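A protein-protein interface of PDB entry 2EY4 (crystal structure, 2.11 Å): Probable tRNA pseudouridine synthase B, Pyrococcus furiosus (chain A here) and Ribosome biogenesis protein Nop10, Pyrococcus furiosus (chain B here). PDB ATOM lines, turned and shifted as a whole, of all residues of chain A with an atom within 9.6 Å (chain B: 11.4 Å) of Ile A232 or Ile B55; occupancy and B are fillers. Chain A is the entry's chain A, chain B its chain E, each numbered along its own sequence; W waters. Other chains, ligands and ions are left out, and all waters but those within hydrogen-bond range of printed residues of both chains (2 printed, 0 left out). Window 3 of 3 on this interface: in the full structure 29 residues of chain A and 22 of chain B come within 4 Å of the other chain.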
ATOM      1  N   ILE A  40     -24.322  21.702  23.031  1.00  0.00           N
ATOM      2  CA  ILE A  40     -24.480  20.288  23.328  1.00  0.00           C
ATOM      3  C   ILE A  40     -24.359  19.976  24.819  1.00  0.00           C
ATOM      4  O   ILE A  40     -25.130  19.183  25.354  1.00  0.00           O
ATOM      5  CB  ILE A  40     -23.460  19.435  22.540  1.00  0.00           C
ATOM      6  CG1 ILE A  40     -23.687  17.953  22.832  1.00  0.00           C
ATOM      7  CG2 ILE A  40     -22.043  19.816  22.943  1.00  0.00           C
ATOM      8  CD1 ILE A  40     -25.048  17.481  22.468  1.00  0.00           C
ATOM      9  N   LEU A 220     -27.183   4.804  21.377  1.00  0.00           N
ATOM     10  CA  LEU A 220     -26.785   5.798  22.368  1.00  0.00           C
ATOM     11  C   LEU A 220     -25.280   5.806  22.579  1.00  0.00           C
ATOM     12  O   LEU A 220     -24.628   6.848  22.419  1.00  0.00           O
ATOM     13  CB  LEU A 220     -27.487   5.551  23.712  1.00  0.00           C
ATOM     14  CG  LEU A 220     -27.316   6.635  24.795  1.00  0.00           C
ATOM     15  CD1 LEU A 220     -27.794   7.981  24.273  1.00  0.00           C
ATOM     16  CD2 LEU A 220     -28.106   6.251  26.041  1.00  0.00           C
ATOM     17  N   VAL A 221     -24.726   4.650  22.936  1.00  0.00           N
ATOM     18  CA  VAL A 221     -23.298   4.550  23.189  1.00  0.00           C
ATOM     19  C   VAL A 221     -22.466   4.934  21.979  1.00  0.00           C
ATOM     20  O   VAL A 221     -21.513   5.706  22.100  1.00  0.00           O
ATOM     21  CB  VAL A 221     -22.893   3.132  23.653  1.00  0.00           C
ATOM     22  CG1 VAL A 221     -23.552   2.818  24.984  1.00  0.00           C
ATOM     23  CG2 VAL A 221     -23.289   2.110  22.611  1.00  0.00           C
ATOM     24  N   ASP A 222     -22.838   4.417  20.812  1.00  0.00           N
ATOM     25  CA  ASP A 222     -22.101   4.716  19.593  1.00  0.00           C
ATOM     26  C   ASP A 222     -22.124   6.198  19.258  1.00  0.00           C
ATOM     27  O   ASP A 222     -21.075   6.784  18.983  1.00  0.00           O
ATOM     28  CB  ASP A 222     -22.644   3.889  18.423  1.00  0.00           C
ATOM     29  CG  ASP A 222     -22.473   2.397  18.645  1.00  0.00           C
ATOM     30  OD1 ASP A 222     -21.703   2.025  19.552  1.00  0.00           O
ATOM     31  OD2 ASP A 222     -23.095   1.599  17.915  1.00  0.00           O
ATOM     32  N   TYR A 223     -23.303   6.814  19.287  1.00  0.00           N
ATOM     33  CA  TYR A 223     -23.388   8.248  18.989  1.00  0.00           C
ATOM     34  C   TYR A 223     -22.543   9.019  19.995  1.00  0.00           C
ATOM     35  O   TYR A 223     -21.900  10.012  19.655  1.00  0.00           O
ATOM     36  CB  TYR A 223     -24.833   8.740  19.044  1.00  0.00           C
ATOM     37  CG  TYR A 223     -25.707   8.147  17.965  1.00  0.00           C
ATOM     38  CD1 TYR A 223     -25.152   7.635  16.785  1.00  0.00           C
ATOM     39  CD2 TYR A 223     -27.092   8.114  18.109  1.00  0.00           C
ATOM     40  CE1 TYR A 223     -25.965   7.106  15.778  1.00  0.00           C
ATOM     41  CE2 TYR A 223     -27.908   7.593  17.110  1.00  0.00           C
ATOM     42  CZ  TYR A 223     -27.341   7.094  15.950  1.00  0.00           C
ATOM     43  OH  TYR A 223     -28.160   6.609  14.962  1.00  0.00           O
ATOM     44  N   TYR A 224     -22.544   8.544  21.235  1.00  0.00           N
ATOM     45  CA  TYR A 224     -21.759   9.170  22.275  1.00  0.00           C
ATOM     46  C   TYR A 224     -20.305   9.115  21.820  1.00  0.00           C
ATOM     47  O   TYR A 224     -19.624  10.144  21.744  1.00  0.00           O
ATOM     48  CB  TYR A 224     -21.922   8.406  23.577  1.00  0.00           C
ATOM     49  CG  TYR A 224     -21.215   9.045  24.735  1.00  0.00           C
ATOM     50  CD1 TYR A 224     -21.584  10.312  25.182  1.00  0.00           C
ATOM     51  CD2 TYR A 224     -20.202   8.374  25.411  1.00  0.00           C
ATOM     52  CE1 TYR A 224     -20.972  10.893  26.275  1.00  0.00           C
ATOM     53  CE2 TYR A 224     -19.577   8.948  26.513  1.00  0.00           C
ATOM     54  CZ  TYR A 224     -19.972  10.214  26.940  1.00  0.00           C
ATOM     55  OH  TYR A 224     -19.372  10.789  28.038  1.00  0.00           O
ATOM     56  N   TYR A 225     -19.835   7.907  21.513  1.00  0.00           N
ATOM     57  CA  TYR A 225     -18.462   7.729  21.048  1.00  0.00           C
ATOM     58  C   TYR A 225     -18.133   8.647  19.865  1.00  0.00           C
ATOM     59  O   TYR A 225     -17.049   9.225  19.804  1.00  0.00           O
ATOM     60  CB  TYR A 225     -18.208   6.272  20.644  1.00  0.00           C
ATOM     61  CG  TYR A 225     -17.821   5.368  21.791  1.00  0.00           C
ATOM     62  CD1 TYR A 225     -18.752   4.985  22.756  1.00  0.00           C
ATOM     63  CD2 TYR A 225     -16.516   4.900  21.917  1.00  0.00           C
ATOM     64  CE1 TYR A 225     -18.395   4.159  23.817  1.00  0.00           C
ATOM     65  CE2 TYR A 225     -16.147   4.070  22.974  1.00  0.00           C
ATOM     66  CZ  TYR A 225     -17.090   3.704  23.918  1.00  0.00           C
ATOM     67  OH  TYR A 225     -16.732   2.875  24.953  1.00  0.00           O
ATOM     68  N   PHE A 226     -19.055   8.782  18.921  1.00  0.00           N
ATOM     69  CA  PHE A 226     -18.804   9.645  17.771  1.00  0.00           C
ATOM     70  C   PHE A 226     -18.506  11.068  18.254  1.00  0.00           C
ATOM     71  O   PHE A 226     -17.590  11.727  17.766  1.00  0.00           O
ATOM     72  CB  PHE A 226     -20.015   9.653  16.830  1.00  0.00           C
ATOM     73  CG  PHE A 226     -20.344   8.307  16.244  1.00  0.00           C
ATOM     74  CD1 PHE A 226     -21.581   8.082  15.647  1.00  0.00           C
ATOM     75  CD2 PHE A 226     -19.428   7.252  16.311  1.00  0.00           C
ATOM     76  CE1 PHE A 226     -21.904   6.825  15.128  1.00  0.00           C
ATOM     77  CE2 PHE A 226     -19.743   5.997  15.797  1.00  0.00           C
ATOM     78  CZ  PHE A 226     -20.986   5.779  15.204  1.00  0.00           C
ATOM     79  N   TRP A 227     -19.280  11.536  19.224  1.00  0.00           N
ATOM     80  CA  TRP A 227     -19.081  12.873  19.758  1.00  0.00           C
ATOM     81  C   TRP A 227     -17.767  12.962  20.542  1.00  0.00           C
ATOM     82  O   TRP A 227     -16.946  13.848  20.300  1.00  0.00           O
ATOM     83  CB  TRP A 227     -20.272  13.269  20.649  1.00  0.00           C
ATOM     84  CG  TRP A 227     -20.059  14.548  21.409  1.00  0.00           C
ATOM     85  CD1 TRP A 227     -19.556  15.712  20.917  1.00  0.00           C
ATOM     86  CD2 TRP A 227     -20.303  14.773  22.805  1.00  0.00           C
ATOM     87  NE1 TRP A 227     -19.460  16.646  21.915  1.00  0.00           N
ATOM     88  CE2 TRP A 227     -19.912  16.098  23.084  1.00  0.00           C
ATOM     89  CE3 TRP A 227     -20.809  13.983  23.843  1.00  0.00           C
ATOM     90  CZ2 TRP A 227     -20.010  16.658  24.367  1.00  0.00           C
ATOM     91  CZ3 TRP A 227     -20.909  14.535  25.121  1.00  0.00           C
ATOM     92  CH2 TRP A 227     -20.510  15.862  25.369  1.00  0.00           C
ATOM     93  N   LYS A 228     -17.556  12.028  21.463  1.00  0.00           N
ATOM     94  CA  LYS A 228     -16.343  12.032  22.266  1.00  0.00           C
ATOM     95  C   LYS A 228     -15.045  11.762  21.497  1.00  0.00           C
ATOM     96  O   LYS A 228     -14.062  12.486  21.663  1.00  0.00           O
ATOM     97  CB  LYS A 228     -16.487  11.039  23.423  1.00  0.00           C
ATOM     98  CG  LYS A 228     -16.672  11.710  24.779  1.00  0.00           C
ATOM     99  CD  LYS A 228     -17.839  12.684  24.768  1.00  0.00           C
ATOM    100  CE  LYS A 228     -18.041  13.361  26.127  1.00  0.00           C
ATOM    101  NZ  LYS A 228     -16.997  14.374  26.457  1.00  0.00           N
ATOM    102  N   GLU A 229     -15.034  10.734  20.655  1.00  0.00           N
ATOM    103  CA  GLU A 229     -13.831  10.395  19.899  1.00  0.00           C
ATOM    104  C   GLU A 229     -13.625  11.196  18.611  1.00  0.00           C
ATOM    105  O   GLU A 229     -12.566  11.782  18.406  1.00  0.00           O
ATOM    106  CB  GLU A 229     -13.827   8.901  19.566  1.00  0.00           C
ATOM    107  CG  GLU A 229     -13.894   7.997  20.787  1.00  0.00           C
ATOM    108  CD  GLU A 229     -13.716   6.523  20.450  1.00  0.00           C
ATOM    109  OE1 GLU A 229     -13.780   5.692  21.380  1.00  0.00           O
ATOM    110  OE2 GLU A 229     -13.511   6.194  19.261  1.00  0.00           O
ATOM    111  N   ASP A 230     -14.641  11.225  17.753  1.00  0.00           N
ATOM    112  CA  ASP A 230     -14.558  11.915  16.467  1.00  0.00           C
ATOM    113  C   ASP A 230     -14.978  13.390  16.477  1.00  0.00           C
ATOM    114  O   ASP A 230     -14.843  14.084  15.470  1.00  0.00           O
ATOM    115  CB  ASP A 230     -15.411  11.159  15.455  1.00  0.00           C
ATOM    116  CG  ASP A 230     -15.223   9.659  15.547  1.00  0.00           C
ATOM    117  OD1 ASP A 230     -16.228   8.932  15.422  1.00  0.00           O
ATOM    118  OD2 ASP A 230     -14.075   9.207  15.745  1.00  0.00           O
ATOM    119  N   GLY A 231     -15.497  13.865  17.603  1.00  0.00           N
ATOM    120  CA  GLY A 231     -15.909  15.254  17.684  1.00  0.00           C
ATOM    121  C   GLY A 231     -17.164  15.580  16.894  1.00  0.00           C
ATOM    122  O   GLY A 231     -17.381  16.740  16.517  1.00  0.00           O
ATOM    123  N   ILE A 232     -17.988  14.566  16.635  1.00  0.00           N
ATOM    124  CA  ILE A 232     -19.241  14.745  15.898  1.00  0.00           C
ATOM    125  C   ILE A 232     -20.388  14.892  16.904  1.00  0.00           C
ATOM    126  O   ILE A 232     -20.694  13.962  17.647  1.00  0.00           O
ATOM    127  CB  ILE A 232     -19.530  13.533  14.978  1.00  0.00           C
ATOM    128  CG1 ILE A 232     -18.404  13.370  13.953  1.00  0.00           C
ATOM    129  CG2 ILE A 232     -20.859  13.714  14.287  1.00  0.00           C
ATOM    130  CD1 ILE A 232     -18.223  14.563  13.029  1.00  0.00           C
ATOM    131  N   GLU A 233     -21.016  16.063  16.919  1.00  0.00           N
ATOM    132  CA  GLU A 233     -22.108  16.349  17.840  1.00  0.00           C
ATOM    133  C   GLU A 233     -23.514  16.059  17.307  1.00  0.00           C
ATOM    134  O   GLU A 233     -24.417  15.711  18.075  1.00  0.00           O
ATOM    135  CB  GLU A 233     -22.047  17.822  18.275  1.00  0.00           C
ATOM    136  CG  GLU A 233     -20.869  18.172  19.178  1.00  0.00           C
ATOM    137  CD  GLU A 233     -20.846  19.640  19.566  1.00  0.00           C
ATOM    138  OE1 GLU A 233     -21.933  20.262  19.592  1.00  0.00           O
ATOM    139  OE2 GLU A 233     -19.747  20.166  19.863  1.00  0.00           O
ATOM    140  N   GLU A 234     -23.702  16.199  15.998  1.00  0.00           N
ATOM    141  CA  GLU A 234     -25.015  16.004  15.401  1.00  0.00           C
ATOM    142  C   GLU A 234     -25.787  14.752  15.815  1.00  0.00           C
ATOM    143  O   GLU A 234     -26.970  14.842  16.149  1.00  0.00           O
ATOM    144  CB  GLU A 234     -24.915  16.074  13.876  1.00  0.00           C
ATOM    145  CG  GLU A 234     -24.049  15.008  13.241  1.00  0.00           C
ATOM    146  CD  GLU A 234     -23.980  15.147  11.733  1.00  0.00           C
ATOM    147  OE1 GLU A 234     -23.422  16.155  11.254  1.00  0.00           O
ATOM    148  OE2 GLU A 234     -24.494  14.250  11.033  1.00  0.00           O
ATOM    149  N   TYR A 235     -25.136  13.591  15.812  1.00  0.00           N
ATOM    150  CA  TYR A 235     -25.826  12.357  16.172  1.00  0.00           C
ATOM    151  C   TYR A 235     -26.200  12.248  17.640  1.00  0.00           C
ATOM    152  O   TYR A 235     -27.331  11.896  17.972  1.00  0.00           O
ATOM    153  CB  TYR A 235     -24.996  11.143  15.747  1.00  0.00           C
ATOM    154  CG  TYR A 235     -24.705  11.144  14.265  1.00  0.00           C
ATOM    155  CD1 TYR A 235     -23.506  11.663  13.770  1.00  0.00           C
ATOM    156  CD2 TYR A 235     -25.663  10.701  13.349  1.00  0.00           C
ATOM    157  CE1 TYR A 235     -23.270  11.747  12.400  1.00  0.00           C
ATOM    158  CE2 TYR A 235     -25.437  10.782  11.979  1.00  0.00           C
ATOM    159  CZ  TYR A 235     -24.239  11.308  11.511  1.00  0.00           C
ATOM    160  OH  TYR A 235     -24.018  11.399  10.154  1.00  0.00           O
ATOM    161  N   PHE A 236     -25.259  12.548  18.527  1.00  0.00           N
ATOM    162  CA  PHE A 236     -25.551  12.471  19.947  1.00  0.00           C
ATOM    163  C   PHE A 236     -26.585  13.539  20.309  1.00  0.00           C
ATOM    164  O   PHE A 236     -27.457  13.303  21.138  1.00  0.00           O
ATOM    165  CB  PHE A 236     -24.276  12.664  20.769  1.00  0.00           C
ATOM    166  CG  PHE A 236     -24.467  12.436  22.238  1.00  0.00           C
ATOM    167  CD1 PHE A 236     -24.939  11.212  22.705  1.00  0.00           C
ATOM    168  CD2 PHE A 236     -24.181  13.442  23.154  1.00  0.00           C
ATOM    169  CE1 PHE A 236     -25.123  10.990  24.066  1.00  0.00           C
ATOM    170  CE2 PHE A 236     -24.359  13.234  24.519  1.00  0.00           C
ATOM    171  CZ  PHE A 236     -24.831  12.009  24.980  1.00  0.00           C
ATOM    172  N   ARG A 237     -26.497  14.707  19.682  1.00  0.00           N
ATOM    173  CA  ARG A 237     -27.452  15.773  19.961  1.00  0.00           C
ATOM    174  C   ARG A 237     -28.869  15.318  19.667  1.00  0.00           C
ATOM    175  O   ARG A 237     -29.777  15.584  20.447  1.00  0.00           O
ATOM    176  CB  ARG A 237     -27.155  17.037  19.140  1.00  0.00           C
ATOM    177  CG  ARG A 237     -28.330  18.022  19.108  1.00  0.00           C
ATOM    178  CD  ARG A 237     -27.984  19.334  18.428  1.00  0.00           C
ATOM    179  NE  ARG A 237     -27.174  20.170  19.299  1.00  0.00           N
ATOM    180  CZ  ARG A 237     -27.660  21.068  20.150  1.00  0.00           C
ATOM    181  NH1 ARG A 237     -28.967  21.272  20.243  1.00  0.00           N
ATOM    182  NH2 ARG A 237     -26.830  21.736  20.934  1.00  0.00           N
ATOM    183  N   LYS A 238     -29.063  14.627  18.549  1.00  0.00           N
ATOM    184  CA  LYS A 238     -30.401  14.165  18.187  1.00  0.00           C
ATOM    185  C   LYS A 238     -30.892  12.994  19.013  1.00  0.00           C
ATOM    186  O   LYS A 238     -32.080  12.718  19.037  1.00  0.00           O
ATOM    187  CB  LYS A 238     -30.472  13.808  16.698  1.00  0.00           C
ATOM    188  CG  LYS A 238     -30.825  14.994  15.824  1.00  0.00           C
ATOM    189  CD  LYS A 238     -29.791  16.099  15.967  1.00  0.00           C
ATOM    190  CE  LYS A 238     -30.400  17.470  15.718  1.00  0.00           C
ATOM    191  NZ  LYS A 238     -31.340  17.854  16.809  1.00  0.00           N
ATOM    192  N   ARG B  45     -18.766  -2.799  15.625  1.00  0.00           N
ATOM    193  CA  ARG B  45     -20.004  -2.169  15.194  1.00  0.00           C
ATOM    194  C   ARG B  45     -19.772  -0.720  14.772  1.00  0.00           C
ATOM    195  O   ARG B  45     -20.271  -0.270  13.742  1.00  0.00           O
ATOM    196  CB  ARG B  45     -21.032  -2.227  16.326  1.00  0.00           C
ATOM    197  CG  ARG B  45     -22.416  -1.731  15.941  1.00  0.00           C
ATOM    198  CD  ARG B  45     -23.388  -1.796  17.123  1.00  0.00           C
ATOM    199  NE  ARG B  45     -22.982  -0.934  18.234  1.00  0.00           N
ATOM    200  CZ  ARG B  45     -22.641  -1.390  19.434  1.00  0.00           C
ATOM    201  NH1 ARG B  45     -22.656  -2.698  19.675  1.00  0.00           N
ATOM    202  NH2 ARG B  45     -22.292  -0.548  20.395  1.00  0.00           N
ATOM    203  N   ARG B  46     -19.007   0.010  15.570  1.00  0.00           N
ATOM    204  CA  ARG B  46     -18.742   1.396  15.258  1.00  0.00           C
ATOM    205  C   ARG B  46     -17.908   1.565  14.002  1.00  0.00           C
ATOM    206  O   ARG B  46     -18.062   2.550  13.282  1.00  0.00           O
ATOM    207  CB  ARG B  46     -18.079   2.087  16.440  1.00  0.00           C
ATOM    208  CG  ARG B  46     -19.048   2.349  17.574  1.00  0.00           C
ATOM    209  CD  ARG B  46     -18.444   3.247  18.646  1.00  0.00           C
ATOM    210  NE  ARG B  46     -18.382   2.562  19.931  1.00  0.00           N
ATOM    211  CZ  ARG B  46     -17.458   1.669  20.249  1.00  0.00           C
ATOM    212  NH1 ARG B  46     -16.516   1.363  19.367  1.00  0.00           N
ATOM    213  NH2 ARG B  46     -17.486   1.067  21.430  1.00  0.00           N
ATOM    214  N   ARG B  47     -17.028   0.606  13.737  1.00  0.00           N
ATOM    215  CA  ARG B  47     -16.196   0.662  12.542  1.00  0.00           C
ATOM    216  C   ARG B  47     -17.093   0.729  11.307  1.00  0.00           C
ATOM    217  O   ARG B  47     -16.944   1.623  10.469  1.00  0.00           O
ATOM    218  CB  ARG B  47     -15.296  -0.574  12.436  1.00  0.00           C
ATOM    219  CG  ARG B  47     -14.242  -0.721  13.511  1.00  0.00           C
ATOM    220  CD  ARG B  47     -13.466  -2.016  13.287  1.00  0.00           C
ATOM    221  NE  ARG B  47     -12.503  -2.308  14.346  1.00  0.00           N
ATOM    222  CZ  ARG B  47     -11.467  -1.534  14.652  1.00  0.00           C
ATOM    223  NH1 ARG B  47     -11.251  -0.411  13.982  1.00  0.00           N
ATOM    224  NH2 ARG B  47     -10.641  -1.891  15.624  1.00  0.00           N
ATOM    225  N   TRP B  48     -18.031  -0.205  11.181  1.00  0.00           N
ATOM    226  CA  TRP B  48     -18.880  -0.144  10.008  1.00  0.00           C
ATOM    227  C   TRP B  48     -19.856   1.019  10.104  1.00  0.00           C
ATOM    228  O   TRP B  48     -20.165   1.661   9.098  1.00  0.00           O
ATOM    229  CB  TRP B  48     -19.610  -1.476   9.746  1.00  0.00           C
ATOM    230  CG  TRP B  48     -20.580  -1.978  10.787  1.00  0.00           C
ATOM    231  CD1 TRP B  48     -20.407  -3.059  11.610  1.00  0.00           C
ATOM    232  CD2 TRP B  48     -21.910  -1.499  11.034  1.00  0.00           C
ATOM    233  NE1 TRP B  48     -21.548  -3.289  12.343  1.00  0.00           N
ATOM    234  CE2 TRP B  48     -22.486  -2.348  12.010  1.00  0.00           C
ATOM    235  CE3 TRP B  48     -22.674  -0.441  10.520  1.00  0.00           C
ATOM    236  CZ2 TRP B  48     -23.793  -2.166  12.487  1.00  0.00           C
ATOM    237  CZ3 TRP B  48     -23.973  -0.262  10.994  1.00  0.00           C
ATOM    238  CH2 TRP B  48     -24.518  -1.123  11.967  1.00  0.00           C
ATOM    239  N   LYS B  49     -20.314   1.319  11.315  1.00  0.00           N
ATOM    240  CA  LYS B  49     -21.254   2.415  11.480  1.00  0.00           C
ATOM    241  C   LYS B  49     -20.617   3.747  11.071  1.00  0.00           C
ATOM    242  O   LYS B  49     -21.251   4.559  10.400  1.00  0.00           O
ATOM    243  CB  LYS B  49     -21.764   2.468  12.922  1.00  0.00           C
ATOM    244  CG  LYS B  49     -23.005   3.337  13.088  1.00  0.00           C
ATOM    245  CD  LYS B  49     -23.711   3.100  14.425  1.00  0.00           C
ATOM    246  CE  LYS B  49     -24.345   1.719  14.496  1.00  0.00           C
ATOM    247  NZ  LYS B  49     -25.169   1.569  15.727  1.00  0.00           N
ATOM    248  N   ARG B  50     -19.364   3.978  11.449  1.00  0.00           N
ATOM    249  CA  ARG B  50     -18.718   5.229  11.059  1.00  0.00           C
ATOM    250  C   ARG B  50     -18.731   5.344   9.545  1.00  0.00           C
ATOM    251  O   ARG B  50     -18.938   6.426   8.988  1.00  0.00           O
ATOM    252  CB  ARG B  50     -17.274   5.297  11.560  1.00  0.00           C
ATOM    253  CG  ARG B  50     -17.145   5.590  13.044  1.00  0.00           C
ATOM    254  CD  ARG B  50     -15.771   6.151  13.373  1.00  0.00           C
ATOM    255  NE  ARG B  50     -15.654   6.522  14.780  1.00  0.00           N
ATOM    256  CZ  ARG B  50     -15.545   5.652  15.782  1.00  0.00           C
ATOM    257  NH1 ARG B  50     -15.532   4.347  15.535  1.00  0.00           N
ATOM    258  NH2 ARG B  50     -15.456   6.089  17.035  1.00  0.00           N
ATOM    259  N   GLU B  51     -18.508   4.215   8.882  1.00  0.00           N
ATOM    260  CA  GLU B  51     -18.492   4.171   7.427  1.00  0.00           C
ATOM    261  C   GLU B  51     -19.832   4.642   6.861  1.00  0.00           C
ATOM    262  O   GLU B  51     -19.899   5.665   6.182  1.00  0.00           O
ATOM    263  CB  GLU B  51     -18.194   2.747   6.949  1.00  0.00           C
ATOM    264  CG  GLU B  51     -17.944   2.631   5.456  1.00  0.00           C
ATOM    265  CD  GLU B  51     -16.742   3.440   4.999  1.00  0.00           C
ATOM    266  OE1 GLU B  51     -15.627   3.196   5.508  1.00  0.00           O
ATOM    267  OE2 GLU B  51     -16.914   4.321   4.129  1.00  0.00           O
ATOM    268  N   VAL B  52     -20.892   3.894   7.150  1.00  0.00           N
ATOM    269  CA  VAL B  52     -22.226   4.234   6.663  1.00  0.00           C
ATOM    270  C   VAL B  52     -22.609   5.694   6.913  1.00  0.00           C
ATOM    271  O   VAL B  52     -23.170   6.351   6.036  1.00  0.00           O
ATOM    272  CB  VAL B  52     -23.304   3.335   7.311  1.00  0.00           C
ATOM    273  CG1 VAL B  52     -24.689   3.746   6.829  1.00  0.00           C
ATOM    274  CG2 VAL B  52     -23.037   1.879   6.968  1.00  0.00           C
ATOM    275  N   LEU B  53     -22.308   6.198   8.107  1.00  0.00           N
ATOM    276  CA  LEU B  53     -22.640   7.577   8.454  1.00  0.00           C
ATOM    277  C   LEU B  53     -21.685   8.583   7.830  1.00  0.00           C
ATOM    278  O   LEU B  53     -22.062   9.728   7.578  1.00  0.00           O
ATOM    279  CB  LEU B  53     -22.648   7.751   9.975  1.00  0.00           C
ATOM    280  CG  LEU B  53     -23.656   6.858  10.703  1.00  0.00           C
ATOM    281  CD1 LEU B  53     -23.568   7.072  12.202  1.00  0.00           C
ATOM    282  CD2 LEU B  53     -25.056   7.166  10.191  1.00  0.00           C
ATOM    283  N   GLY B  54     -20.452   8.154   7.583  1.00  0.00           N
ATOM    284  CA  GLY B  54     -19.467   9.039   6.991  1.00  0.00           C
ATOM    285  C   GLY B  54     -18.691   9.843   8.017  1.00  0.00           C
ATOM    286  O   GLY B  54     -18.491  11.047   7.849  1.00  0.00           O
ATOM    287  N   ILE B  55     -18.245   9.178   9.079  1.00  0.00           N
ATOM    288  CA  ILE B  55     -17.487   9.841  10.135  1.00  0.00           C
ATOM    289  C   ILE B  55     -16.019   9.414  10.078  1.00  0.00           C
ATOM    290  O   ILE B  55     -15.749   8.369   9.453  1.00  0.00           O
ATOM    291  CB  ILE B  55     -18.068   9.486  11.524  1.00  0.00           C
ATOM    292  CG1 ILE B  55     -19.559   9.838  11.563  1.00  0.00           C
ATOM    293  CG2 ILE B  55     -17.309  10.222  12.611  1.00  0.00           C
ATOM    294  CD1 ILE B  55     -20.247   9.492  12.861  1.00  0.00           C
ATOM    295  OXT ILE B  55     -15.158  10.113  10.659  1.00  0.00           O
HETATM  296  O   HOH W   1     -26.735   3.772  15.616  1.00  0.00           O
HETATM  297  O   HOH W   2     -14.963   3.278  18.422  1.00  0.00           O
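The side-chain carboxylate (OD2) of Asp A222 lies within salt-bridge range of the side-chain amino group (NZ) of Lys B49 (3.0 Å).
The side-chain carboxylate (OD1) of Asp A222 lies within salt-bridge range of the guanidinium group (NE) of Arg B46, 3.4 Å away.
The guanidinium group of Arg B50 lies within salt-bridge range of the side-chain carboxylate of Asp A230 (2.6 Å).
The guanidinium group (NH2) of Arg B50 is in salt-bridge range of the side-chain carboxylate (OE2) of Glu A229 (3.0 Å).
The side-chain carboxylate (OD2) of Asp A222 is in salt-bridge range of the guanidinium group (NE) of Arg B45 (2.6 Å).
Of the 11 printed residues of chain B, 6 touch a printed residue of chain A.
Ile B55 touches four residues of chain A.
Of the printed residues of chain B, Phe A226 touches Lys B49 (3.8 Å), Arg B50 (3.8 Å), Leu B53 (3.4 Å) and Ile B55 (3.4 Å).
Of chain B, only Arg B50 (2.6 Å) and Ile B55 (3.3 Å) come within 4 Å of Asp A230.
No residue of chain B comes within 4 Å of Gly A231.
No residue of chain B comes within 4 Å of Glu A233.
No residue of chain B comes within 4 Å of Glu A234.
Tyr A235 touches two residues of chain B.
Gly B54 touches none of the printed residues of chain A.
Of the printed residues of chain B, Tyr A225 touches Arg B46.
Of the printed residues of chain B, Val A221 touches Arg B45 (3.6 Å).
Of the printed residues of chain A, Lys B49 touches Asp A222 (3.0 Å) and Phe A226 (3.8 Å).
Of the printed residues of chain A, Arg B50 touches Phe A226 (3.8 Å), Glu A229 (3.0 Å) and Asp A230 (2.6 Å).
Of the printed residues of chain B, Asp A222 touches Arg B45, Arg B46 and Lys B49.
Tyr A224 touches none of the printed residues of chain B.
Arg B45 touches Val A221.
CG of Tyr A225 touches NE of Arg B46, 3.4 Å away.
Phe A226 touches Lys B49 (CZ to CG, 3.8 Å).
Phe A226 touches Arg B50.
Phe A226 touches Leu B53.
Ile B55 touches Phe A226.
OD1 of Asp A230 touches CG2 of Ile B55, 3.3 Å away.
Ile B55 touches Ile A232 (CG2 to CG1, 3.6 Å).
Leu B53 touches Tyr A235.
Ile B55 touches Tyr A235 (CD1 to CE1, 3.8 Å).
Water W2 lies within hydrogen-bond range of the guanidinium group (NH1) of Arg B46 (2.6 Å), the guanidinium group (NH1) of Arg B50 (3.1 Å) and the side-chain carboxylate (OE2) of Glu A229 (3.4 Å).
Water W1 bridges NZ of Lys B49 and OH of Tyr A223.
The backbone NH (N) of Trp A227 lies close to the backbone carbonyl oxygen (O) of Ile A232.
N of Gly A231 is in hydrogen-bond range of O of Phe A226.
The backbone carbonyl oxygen of Arg B50 is in hydrogen-bond range of the backbone NH of Ile B55.
The side-chain carboxylate of Glu A234 lies close to the side-chain hydroxyl of Tyr A235 (3.0 Å).
The backbone carbonyl oxygen of Phe A226 is in hydrogen-bond range of the backbone NH of Ile A232 (3.1 Å).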
